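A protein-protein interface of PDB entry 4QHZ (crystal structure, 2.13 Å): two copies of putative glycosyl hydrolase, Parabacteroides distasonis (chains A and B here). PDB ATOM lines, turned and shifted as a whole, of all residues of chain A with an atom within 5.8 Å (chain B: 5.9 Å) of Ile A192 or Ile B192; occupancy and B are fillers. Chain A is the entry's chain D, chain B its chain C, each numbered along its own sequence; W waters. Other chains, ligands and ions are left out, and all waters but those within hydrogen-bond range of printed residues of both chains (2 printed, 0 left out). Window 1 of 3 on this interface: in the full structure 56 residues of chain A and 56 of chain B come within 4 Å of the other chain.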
ATOM      1  N   GLN A  98     -11.511   2.077   1.080  1.00  0.00           N
ATOM      2  CA  GLN A  98     -10.886   2.832   0.025  1.00  0.00           C
ATOM      3  C   GLN A  98     -10.638   1.860  -1.112  1.00  0.00           C
ATOM      4  O   GLN A  98     -10.238   0.721  -0.876  1.00  0.00           O
ATOM      5  CB  GLN A  98      -9.581   3.421   0.523  1.00  0.00           C
ATOM      6  CG  GLN A  98      -8.624   3.817  -0.571  1.00  0.00           C
ATOM      7  CD  GLN A  98      -7.283   4.258  -0.050  1.00  0.00           C
ATOM      8  OE1 GLN A  98      -6.889   3.945   1.079  1.00  0.00           O
ATOM      9  NE2 GLN A  98      -6.578   5.007  -0.865  1.00  0.00           N
ATOM     10  N   VAL A 167      -8.621   6.466 -14.310  1.00  0.00           N
ATOM     11  CA  VAL A 167      -8.269   6.010 -12.975  1.00  0.00           C
ATOM     12  C   VAL A 167      -9.279   6.502 -11.951  1.00  0.00           C
ATOM     13  O   VAL A 167      -9.483   7.704 -11.822  1.00  0.00           O
ATOM     14  CB  VAL A 167      -6.871   6.525 -12.587  1.00  0.00           C
ATOM     15  CG1 VAL A 167      -6.489   6.064 -11.191  1.00  0.00           C
ATOM     16  CG2 VAL A 167      -5.841   6.051 -13.607  1.00  0.00           C
ATOM     17  N   TYR A 168      -9.910   5.575 -11.236  1.00  0.00           N
ATOM     18  CA  TYR A 168     -10.779   5.925 -10.114  1.00  0.00           C
ATOM     19  C   TYR A 168     -10.087   5.621  -8.790  1.00  0.00           C
ATOM     20  O   TYR A 168      -9.527   4.537  -8.606  1.00  0.00           O
ATOM     21  CB  TYR A 168     -12.100   5.149 -10.148  1.00  0.00           C
ATOM     22  CG  TYR A 168     -13.220   5.682 -11.016  1.00  0.00           C
ATOM     23  CD1 TYR A 168     -13.132   6.894 -11.704  1.00  0.00           C
ATOM     24  CD2 TYR A 168     -14.419   4.965 -11.112  1.00  0.00           C
ATOM     25  CE1 TYR A 168     -14.194   7.352 -12.478  1.00  0.00           C
ATOM     26  CE2 TYR A 168     -15.479   5.417 -11.870  1.00  0.00           C
ATOM     27  CZ  TYR A 168     -15.367   6.604 -12.558  1.00  0.00           C
ATOM     28  OH  TYR A 168     -16.443   7.034 -13.315  1.00  0.00           O
ATOM     29  N   ASP A 169     -10.136   6.585  -7.882  1.00  0.00           N
ATOM     30  CA  ASP A 169      -9.863   6.365  -6.472  1.00  0.00           C
ATOM     31  C   ASP A 169     -11.125   6.753  -5.711  1.00  0.00           C
ATOM     32  O   ASP A 169     -11.660   7.843  -5.894  1.00  0.00           O
ATOM     33  CB  ASP A 169      -8.644   7.162  -6.023  1.00  0.00           C
ATOM     34  CG  ASP A 169      -7.346   6.537  -6.512  1.00  0.00           C
ATOM     35  OD1 ASP A 169      -7.029   5.415  -6.056  1.00  0.00           O
ATOM     36  OD2 ASP A 169      -6.652   7.148  -7.348  1.00  0.00           O
ATOM     37  N   ILE A 170     -11.597   5.840  -4.872  1.00  0.00           N
ATOM     38  CA  ILE A 170     -12.891   5.956  -4.228  1.00  0.00           C
ATOM     39  C   ILE A 170     -12.729   5.749  -2.727  1.00  0.00           C
ATOM     40  O   ILE A 170     -12.121   4.773  -2.300  1.00  0.00           O
ATOM     41  CB  ILE A 170     -13.871   4.918  -4.798  1.00  0.00           C
ATOM     42  CG1 ILE A 170     -14.172   5.234  -6.272  1.00  0.00           C
ATOM     43  CG2 ILE A 170     -15.162   4.881  -3.989  1.00  0.00           C
ATOM     44  CD1 ILE A 170     -14.896   4.131  -7.020  1.00  0.00           C
ATOM     45  N   ILE A 171     -13.281   6.666  -1.939  1.00  0.00           N
ATOM     46  CA  ILE A 171     -13.303   6.539  -0.488  1.00  0.00           C
ATOM     47  C   ILE A 171     -14.762   6.501  -0.059  1.00  0.00           C
ATOM     48  O   ILE A 171     -15.518   7.424  -0.361  1.00  0.00           O
ATOM     49  CB  ILE A 171     -12.576   7.706   0.204  1.00  0.00           C
ATOM     50  CG1 ILE A 171     -11.169   7.874  -0.379  1.00  0.00           C
ATOM     51  CG2 ILE A 171     -12.521   7.472   1.711  1.00  0.00           C
ATOM     52  CD1 ILE A 171     -10.444   9.106   0.114  1.00  0.00           C
ATOM     53  N   THR A 190     -16.297   9.804  -1.711  1.00  0.00           N
ATOM     54  CA  THR A 190     -15.448  10.697  -2.482  1.00  0.00           C
ATOM     55  C   THR A 190     -14.935   9.925  -3.686  1.00  0.00           C
ATOM     56  O   THR A 190     -14.545   8.761  -3.557  1.00  0.00           O
ATOM     57  CB  THR A 190     -14.287  11.238  -1.625  1.00  0.00           C
ATOM     58  OG1 THR A 190     -14.805  12.182  -0.689  1.00  0.00           O
ATOM     59  CG2 THR A 190     -13.225  11.927  -2.475  1.00  0.00           C
ATOM     60  N   VAL A 191     -14.998  10.548  -4.860  1.00  0.00           N
ATOM     61  CA  VAL A 191     -14.583   9.912  -6.106  1.00  0.00           C
ATOM     62  C   VAL A 191     -13.609  10.829  -6.819  1.00  0.00           C
ATOM     63  O   VAL A 191     -13.904  12.003  -7.038  1.00  0.00           O
ATOM     64  CB  VAL A 191     -15.779   9.613  -7.041  1.00  0.00           C
ATOM     65  CG1 VAL A 191     -15.303   9.006  -8.353  1.00  0.00           C
ATOM     66  CG2 VAL A 191     -16.770   8.675  -6.378  1.00  0.00           C
ATOM     67  N   ILE A 192     -12.454  10.285  -7.173  1.00  0.00           N
ATOM     68  CA  ILE A 192     -11.416  11.023  -7.872  1.00  0.00           C
ATOM     69  C   ILE A 192     -11.125  10.309  -9.184  1.00  0.00           C
ATOM     70  O   ILE A 192     -10.817   9.115  -9.175  1.00  0.00           O
ATOM     71  CB  ILE A 192     -10.123  11.113  -7.031  1.00  0.00           C
ATOM     72  CG1 ILE A 192     -10.428  11.598  -5.609  1.00  0.00           C
ATOM     73  CG2 ILE A 192      -9.108  12.040  -7.687  1.00  0.00           C
ATOM     74  CD1 ILE A 192      -9.245  11.527  -4.667  1.00  0.00           C
ATOM     75  N   GLN A 193     -11.237  11.022 -10.303  1.00  0.00           N
ATOM     76  CA  GLN A 193     -10.974  10.443 -11.617  1.00  0.00           C
ATOM     77  C   GLN A 193      -9.781  11.120 -12.278  1.00  0.00           C
ATOM     78  O   GLN A 193      -9.793  12.336 -12.515  1.00  0.00           O
ATOM     79  CB  GLN A 193     -12.186  10.543 -12.539  1.00  0.00           C
ATOM     80  CG  GLN A 193     -11.919   9.924 -13.907  1.00  0.00           C
ATOM     81  CD  GLN A 193     -13.085  10.029 -14.866  1.00  0.00           C
ATOM     82  OE1 GLN A 193     -14.201  10.384 -14.487  1.00  0.00           O
ATOM     83  NE2 GLN A 193     -12.832   9.694 -16.125  1.00  0.00           N
ATOM     84  N   ASN A 194      -8.767  10.321 -12.595  1.00  0.00           N
ATOM     85  CA  ASN A 194      -7.535  10.830 -13.187  1.00  0.00           C
ATOM     86  C   ASN A 194      -6.991  12.023 -12.401  1.00  0.00           C
ATOM     87  O   ASN A 194      -6.564  13.028 -12.977  1.00  0.00           O
ATOM     88  CB  ASN A 194      -7.764  11.194 -14.654  1.00  0.00           C
ATOM     89  CG  ASN A 194      -8.243  10.015 -15.464  1.00  0.00           C
ATOM     90  OD1 ASN A 194      -7.714   8.912 -15.330  1.00  0.00           O
ATOM     91  ND2 ASN A 194      -9.243  10.235 -16.313  1.00  0.00           N
ATOM     92  N   GLY A 195      -7.041  11.895 -11.078  1.00  0.00           N
ATOM     93  CA  GLY A 195      -6.546  12.920 -10.172  1.00  0.00           C
ATOM     94  C   GLY A 195      -7.495  14.078  -9.909  1.00  0.00           C
ATOM     95  O   GLY A 195      -7.181  14.943  -9.092  1.00  0.00           O
ATOM     96  N   VAL A 196      -8.642  14.105 -10.592  1.00  0.00           N
ATOM     97  CA  VAL A 196      -9.614  15.182 -10.447  1.00  0.00           C
ATOM     98  C   VAL A 196     -10.777  14.737  -9.565  1.00  0.00           C
ATOM     99  O   VAL A 196     -11.407  13.717  -9.838  1.00  0.00           O
ATOM    100  CB  VAL A 196     -10.152  15.631 -11.826  1.00  0.00           C
ATOM    101  CG1 VAL A 196     -11.138  16.782 -11.690  1.00  0.00           C
ATOM    102  CG2 VAL A 196      -9.004  16.033 -12.740  1.00  0.00           C
ATOM    103  N   VAL A 197     -11.097  15.527  -8.541  1.00  0.00           N
ATOM    104  CA  VAL A 197     -12.223  15.215  -7.652  1.00  0.00           C
ATOM    105  C   VAL A 197     -13.550  15.414  -8.374  1.00  0.00           C
ATOM    106  O   VAL A 197     -13.847  16.508  -8.851  1.00  0.00           O
ATOM    107  CB  VAL A 197     -12.251  16.081  -6.380  1.00  0.00           C
ATOM    108  CG1 VAL A 197     -13.430  15.688  -5.503  1.00  0.00           C
ATOM    109  CG2 VAL A 197     -10.967  15.930  -5.587  1.00  0.00           C
ATOM    110  N   LEU A 198     -14.345  14.348  -8.425  1.00  0.00           N
ATOM    111  CA  LEU A 198     -15.654  14.356  -9.089  1.00  0.00           C
ATOM    112  C   LEU A 198     -16.812  14.318  -8.083  1.00  0.00           C
ATOM    113  O   LEU A 198     -17.871  14.884  -8.327  1.00  0.00           O
ATOM    114  CB  LEU A 198     -15.748  13.173 -10.053  1.00  0.00           C
ATOM    115  CG  LEU A 198     -15.484  13.462 -11.534  1.00  0.00           C
ATOM    116  CD1 LEU A 198     -14.201  14.239 -11.781  1.00  0.00           C
ATOM    117  CD2 LEU A 198     -15.479  12.155 -12.317  1.00  0.00           C
ATOM    118  N   GLN A 199     -16.606  13.627  -6.966  1.00  0.00           N
ATOM    119  CA  GLN A 199     -17.532  13.642  -5.845  1.00  0.00           C
ATOM    120  C   GLN A 199     -16.737  13.983  -4.600  1.00  0.00           C
ATOM    121  O   GLN A 199     -15.810  13.263  -4.237  1.00  0.00           O
ATOM    122  CB  GLN A 199     -18.219  12.292  -5.674  1.00  0.00           C
ATOM    123  CG  GLN A 199     -19.026  11.840  -6.879  1.00  0.00           C
ATOM    124  CD  GLN A 199     -20.283  12.653  -7.103  1.00  0.00           C
ATOM    125  OE1 GLN A 199     -20.770  13.358  -6.206  1.00  0.00           O
ATOM    126  NE2 GLN A 199     -20.832  12.548  -8.307  1.00  0.00           N
ATOM    127  N   GLN B  98      -8.559  21.414  -4.034  1.00  0.00           N
ATOM    128  CA  GLN B  98      -7.863  20.153  -4.141  1.00  0.00           C
ATOM    129  C   GLN B  98      -6.422  20.478  -4.495  1.00  0.00           C
ATOM    130  O   GLN B  98      -6.172  21.358  -5.307  1.00  0.00           O
ATOM    131  CB  GLN B  98      -8.508  19.313  -5.219  1.00  0.00           C
ATOM    132  CG  GLN B  98      -7.641  18.201  -5.745  1.00  0.00           C
ATOM    133  CD  GLN B  98      -8.265  17.478  -6.910  1.00  0.00           C
ATOM    134  OE1 GLN B  98      -9.147  17.993  -7.601  1.00  0.00           O
ATOM    135  NE2 GLN B  98      -7.797  16.272  -7.143  1.00  0.00           N
ATOM    136  N   VAL B 167       3.890  11.100  -2.210  1.00  0.00           N
ATOM    137  CA  VAL B 167       2.872  11.814  -2.965  1.00  0.00           C
ATOM    138  C   VAL B 167       1.700  12.157  -2.065  1.00  0.00           C
ATOM    139  O   VAL B 167       1.094  11.266  -1.479  1.00  0.00           O
ATOM    140  CB  VAL B 167       2.372  10.960  -4.143  1.00  0.00           C
ATOM    141  CG1 VAL B 167       1.289  11.691  -4.920  1.00  0.00           C
ATOM    142  CG2 VAL B 167       3.528  10.592  -5.057  1.00  0.00           C
ATOM    143  N   TYR B 168       1.392  13.447  -1.949  1.00  0.00           N
ATOM    144  CA  TYR B 168       0.202  13.893  -1.235  1.00  0.00           C
ATOM    145  C   TYR B 168      -0.871  14.342  -2.218  1.00  0.00           C
ATOM    146  O   TYR B 168      -0.592  15.103  -3.152  1.00  0.00           O
ATOM    147  CB  TYR B 168       0.502  15.064  -0.293  1.00  0.00           C
ATOM    148  CG  TYR B 168       1.053  14.755   1.093  1.00  0.00           C
ATOM    149  CD1 TYR B 168       1.212  13.455   1.567  1.00  0.00           C
ATOM    150  CD2 TYR B 168       1.375  15.801   1.953  1.00  0.00           C
ATOM    151  CE1 TYR B 168       1.702  13.215   2.850  1.00  0.00           C
ATOM    152  CE2 TYR B 168       1.854  15.575   3.227  1.00  0.00           C
ATOM    153  CZ  TYR B 168       2.009  14.282   3.678  1.00  0.00           C
ATOM    154  OH  TYR B 168       2.501  14.082   4.954  1.00  0.00           O
ATOM    155  N   ASP B 169      -2.092  13.863  -1.998  1.00  0.00           N
ATOM    156  CA  ASP B 169      -3.288  14.446  -2.602  1.00  0.00           C
ATOM    157  C   ASP B 169      -4.186  14.890  -1.460  1.00  0.00           C
ATOM    158  O   ASP B 169      -4.461  14.117  -0.542  1.00  0.00           O
ATOM    159  CB  ASP B 169      -3.981  13.449  -3.525  1.00  0.00           C
ATOM    160  CG  ASP B 169      -3.246  13.284  -4.842  1.00  0.00           C
ATOM    161  OD1 ASP B 169      -3.198  14.266  -5.611  1.00  0.00           O
ATOM    162  OD2 ASP B 169      -2.686  12.194  -5.102  1.00  0.00           O
ATOM    163  N   ILE B 170      -4.613  16.150  -1.511  1.00  0.00           N
ATOM    164  CA  ILE B 170      -5.285  16.803  -0.394  1.00  0.00           C
ATOM    165  C   ILE B 170      -6.572  17.461  -0.884  1.00  0.00           C
ATOM    166  O   ILE B 170      -6.554  18.182  -1.878  1.00  0.00           O
ATOM    167  CB  ILE B 170      -4.377  17.865   0.244  1.00  0.00           C
ATOM    168  CG1 ILE B 170      -3.165  17.193   0.900  1.00  0.00           C
ATOM    169  CG2 ILE B 170      -5.150  18.699   1.256  1.00  0.00           C
ATOM    170  CD1 ILE B 170      -2.060  18.150   1.318  1.00  0.00           C
ATOM    171  N   ILE B 171      -7.678  17.181  -0.202  1.00  0.00           N
ATOM    172  CA  ILE B 171      -8.958  17.802  -0.507  1.00  0.00           C
ATOM    173  C   ILE B 171      -9.390  18.561   0.733  1.00  0.00           C
ATOM    174  O   ILE B 171      -9.505  17.968   1.805  1.00  0.00           O
ATOM    175  CB  ILE B 171     -10.031  16.770  -0.896  1.00  0.00           C
ATOM    176  CG1 ILE B 171      -9.518  15.861  -2.021  1.00  0.00           C
ATOM    177  CG2 ILE B 171     -11.320  17.478  -1.312  1.00  0.00           C
ATOM    178  CD1 ILE B 171     -10.438  14.697  -2.346  1.00  0.00           C
ATOM    179  N   THR B 190      -9.235  15.789   3.614  1.00  0.00           N
ATOM    180  CA  THR B 190      -8.856  14.428   3.294  1.00  0.00           C
ATOM    181  C   THR B 190      -7.422  14.464   2.788  1.00  0.00           C
ATOM    182  O   THR B 190      -7.070  15.322   1.981  1.00  0.00           O
ATOM    183  CB  THR B 190      -9.823  13.802   2.257  1.00  0.00           C
ATOM    184  OG1 THR B 190     -11.083  13.536   2.891  1.00  0.00           O
ATOM    185  CG2 THR B 190      -9.285  12.499   1.685  1.00  0.00           C
ATOM    186  N   VAL B 191      -6.594  13.548   3.290  1.00  0.00           N
ATOM    187  CA  VAL B 191      -5.190  13.464   2.908  1.00  0.00           C
ATOM    188  C   VAL B 191      -4.869  12.044   2.470  1.00  0.00           C
ATOM    189  O   VAL B 191      -5.150  11.089   3.195  1.00  0.00           O
ATOM    190  CB  VAL B 191      -4.255  13.862   4.073  1.00  0.00           C
ATOM    191  CG1 VAL B 191      -2.793  13.722   3.667  1.00  0.00           C
ATOM    192  CG2 VAL B 191      -4.533  15.286   4.530  1.00  0.00           C
ATOM    193  N   ILE B 192      -4.283  11.917   1.284  1.00  0.00           N
ATOM    194  CA  ILE B 192      -3.903  10.631   0.724  1.00  0.00           C
ATOM    195  C   ILE B 192      -2.408  10.654   0.448  1.00  0.00           C
ATOM    196  O   ILE B 192      -1.932  11.543  -0.248  1.00  0.00           O
ATOM    197  CB  ILE B 192      -4.669  10.340  -0.586  1.00  0.00           C
ATOM    198  CG1 ILE B 192      -6.179  10.549  -0.398  1.00  0.00           C
ATOM    199  CG2 ILE B 192      -4.403   8.913  -1.071  1.00  0.00           C
ATOM    200  CD1 ILE B 192      -6.977  10.471  -1.685  1.00  0.00           C
ATOM    201  N   GLN B 193      -1.669   9.700   1.018  1.00  0.00           N
ATOM    202  CA  GLN B 193      -0.227   9.622   0.822  1.00  0.00           C
ATOM    203  C   GLN B 193       0.156   8.339   0.098  1.00  0.00           C
ATOM    204  O   GLN B 193      -0.117   7.232   0.581  1.00  0.00           O
ATOM    205  CB  GLN B 193       0.542   9.694   2.148  1.00  0.00           C
ATOM    206  CG  GLN B 193       2.051   9.632   1.939  1.00  0.00           C
ATOM    207  CD  GLN B 193       2.853   9.678   3.224  1.00  0.00           C
ATOM    208  OE1 GLN B 193       2.323   9.939   4.303  1.00  0.00           O
ATOM    209  NE2 GLN B 193       4.152   9.418   3.110  1.00  0.00           N
ATOM    210  N   ASN B 194       0.799   8.497  -1.051  1.00  0.00           N
ATOM    211  CA  ASN B 194       1.174   7.361  -1.889  1.00  0.00           C
ATOM    212  C   ASN B 194      -0.004   6.416  -2.111  1.00  0.00           C
ATOM    213  O   ASN B 194       0.136   5.189  -2.041  1.00  0.00           O
ATOM    214  CB  ASN B 194       2.369   6.627  -1.280  1.00  0.00           C
ATOM    215  CG  ASN B 194       3.572   7.534  -1.107  1.00  0.00           C
ATOM    216  OD1 ASN B 194       3.902   8.312  -2.005  1.00  0.00           O
ATOM    217  ND2 ASN B 194       4.224   7.453   0.048  1.00  0.00           N
ATOM    218  N   GLY B 195      -1.164   7.012  -2.374  1.00  0.00           N
ATOM    219  CA  GLY B 195      -2.387   6.266  -2.630  1.00  0.00           C
ATOM    220  C   GLY B 195      -3.120   5.748  -1.401  1.00  0.00           C
ATOM    221  O   GLY B 195      -4.209   5.193  -1.537  1.00  0.00           O
ATOM    222  N   VAL B 196      -2.545   5.946  -0.210  1.00  0.00           N
ATOM    223  CA  VAL B 196      -3.138   5.480   1.038  1.00  0.00           C
ATOM    224  C   VAL B 196      -3.811   6.629   1.789  1.00  0.00           C
ATOM    225  O   VAL B 196      -3.182   7.654   2.045  1.00  0.00           O
ATOM    226  CB  VAL B 196      -2.076   4.834   1.944  1.00  0.00           C
ATOM    227  CG1 VAL B 196      -2.704   4.297   3.224  1.00  0.00           C
ATOM    228  CG2 VAL B 196      -1.354   3.712   1.208  1.00  0.00           C
ATOM    229  N   VAL B 197      -5.081   6.452   2.157  1.00  0.00           N
ATOM    230  CA  VAL B 197      -5.813   7.478   2.902  1.00  0.00           C
ATOM    231  C   VAL B 197      -5.268   7.585   4.327  1.00  0.00           C
ATOM    232  O   VAL B 197      -5.281   6.609   5.079  1.00  0.00           O
ATOM    233  CB  VAL B 197      -7.321   7.208   2.993  1.00  0.00           C
ATOM    234  CG1 VAL B 197      -8.014   8.323   3.768  1.00  0.00           C
ATOM    235  CG2 VAL B 197      -7.943   7.110   1.618  1.00  0.00           C
ATOM    236  N   LEU B 198      -4.828   8.787   4.686  1.00  0.00           N
ATOM    237  CA  LEU B 198      -4.272   9.066   6.010  1.00  0.00           C
ATOM    238  C   LEU B 198      -5.224   9.904   6.866  1.00  0.00           C
ATOM    239  O   LEU B 198      -5.249   9.765   8.090  1.00  0.00           O
ATOM    240  CB  LEU B 198      -2.919   9.767   5.863  1.00  0.00           C
ATOM    241  CG  LEU B 198      -1.666   8.891   6.005  1.00  0.00           C
ATOM    242  CD1 LEU B 198      -1.702   7.635   5.149  1.00  0.00           C
ATOM    243  CD2 LEU B 198      -0.423   9.718   5.685  1.00  0.00           C
ATOM    244  N   GLN B 199      -5.965  10.804   6.222  1.00  0.00           N
ATOM    245  CA  GLN B 199      -7.024  11.563   6.872  1.00  0.00           C
ATOM    246  C   GLN B 199      -8.274  11.394   6.029  1.00  0.00           C
ATOM    247  O   GLN B 199      -8.289  11.772   4.855  1.00  0.00           O
ATOM    248  CB  GLN B 199      -6.668  13.041   6.997  1.00  0.00           C
ATOM    249  CG  GLN B 199      -5.412  13.316   7.810  1.00  0.00           C
ATOM    250  CD  GLN B 199      -5.570  13.042   9.294  1.00  0.00           C
ATOM    251  OE1 GLN B 199      -6.683  12.962   9.816  1.00  0.00           O
ATOM    252  NE2 GLN B 199      -4.444  12.923   9.985  1.00  0.00           N
HETATM  253  O   HOH W   1      -4.662  13.835  -7.753  1.00  0.00           O
HETATM  254  O   HOH W   2      -4.827   5.618  -4.458  1.00  0.00           O
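NE2 of Gln B98 sits at hydrogen-bond distance from O of Gly A195, 2.4 Å away.
N of Val A197 sits at hydrogen-bond distance from OE1 of Gln B98.
O of Gly B195 lies within hydrogen-bond range of NE2 of Gln A98 (2.5 Å).
The side-chain amide oxygen of Gln A98 is in hydrogen-bond range of the backbone NH of Val B197 (3.3 Å).
The backbone carbonyl oxygen of Asp B169 lies within hydrogen-bond range of the backbone NH of Ile B192, 2.9 Å away.
O of Ile B171 lies within hydrogen-bond range of N of Thr B190, at 2.8 Å.
The backbone NH of Ile A192 lies within hydrogen-bond range of the backbone carbonyl oxygen of Asp A169 (2.9 Å).
The backbone carbonyl oxygen of Ile A171 sits at hydrogen-bond distance from the backbone NH of Thr A190.
CA of Val B196 touches NE2 of Gln A98, 3.96 Å away.
Ile A171 touches Thr B190.
Ile A171 touches Val B197.
Ile B171 touches Thr A190 (CD1 to CG2, 3.9 Å).
Ile A192 touches Ile B192 (CD1 to CD1, 3.9 Å).
Val A196 touches Gln B98.
Ile B171 touches Val A197.
Of the printed residues of chain B, Ile A171 touches Thr B190 (3.9 Å) and Val B197 (3.5 Å).
Ile A192 touches just one residue of chain B: Ile B192.
Printed residues of chain B within 4 Å of Val A196: Gln B98.
Of the printed residues of chain A, Gln B98 touches Gly A195 (2.4 Å), Val A196 (3.9 Å) and Val A197 (3.3 Å).
Of chain A, only Ile A192 (3.9 Å) comes within 4 Å of Ile B192.
The nearest residue of chain B that does not touch Ile A192 is Ile B171 (4.1 Å).
The nearest printed residue of chain A that does not touch Gln B98 is Ile A192 (4.5 Å).
Printed residues of chain B that touch a printed residue of chain A: Gln B98, Ile B171, Thr B190, Ile B192, Gly B195, Val B196 and Val B197.
Hydrophobic or aromatic side chains of chain B that line the printed part of chain A: Ile B171, Ile B192 and Val B197.
Printed residues of chain A that touch a printed residue of chain B: Gln A98, Ile A171, Thr A190, Ile A192, Gly A195, Val A196 and Val A197.
Hydrophobic or aromatic side chains of chain A that line the printed part of chain B: Ile A171, Ile A192 and Val A197.
Among the printed residues, 11 pairs touch across the chains.
Gln A98 touches Gly B195, and with the chains exchanged Gly A195 touches Gln B98.
Gln A98 touches Val B196, and with the chains exchanged Val A196 touches Gln B98.
Ile A171 touches Val B197, and with the chains exchanged Val A197 touches Ile B171.
Ile B192 touches its own counterpart, Ile A192.
Positions printed for both chains: 98, 167, 168, 169, 170, 171, 190, 191, 192, 193, 194, 195, 196, 197, 198 and 199.
Water W1 lies within hydrogen-bond range of OD1 of Asp B169 (2.6 Å) and O of Gly A195 (3.1 Å).
Water W2 lies within hydrogen-bond range of the side-chain carboxylate (OD1) of Asp A169 and the backbone carbonyl oxygen (O) of Gly B195.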
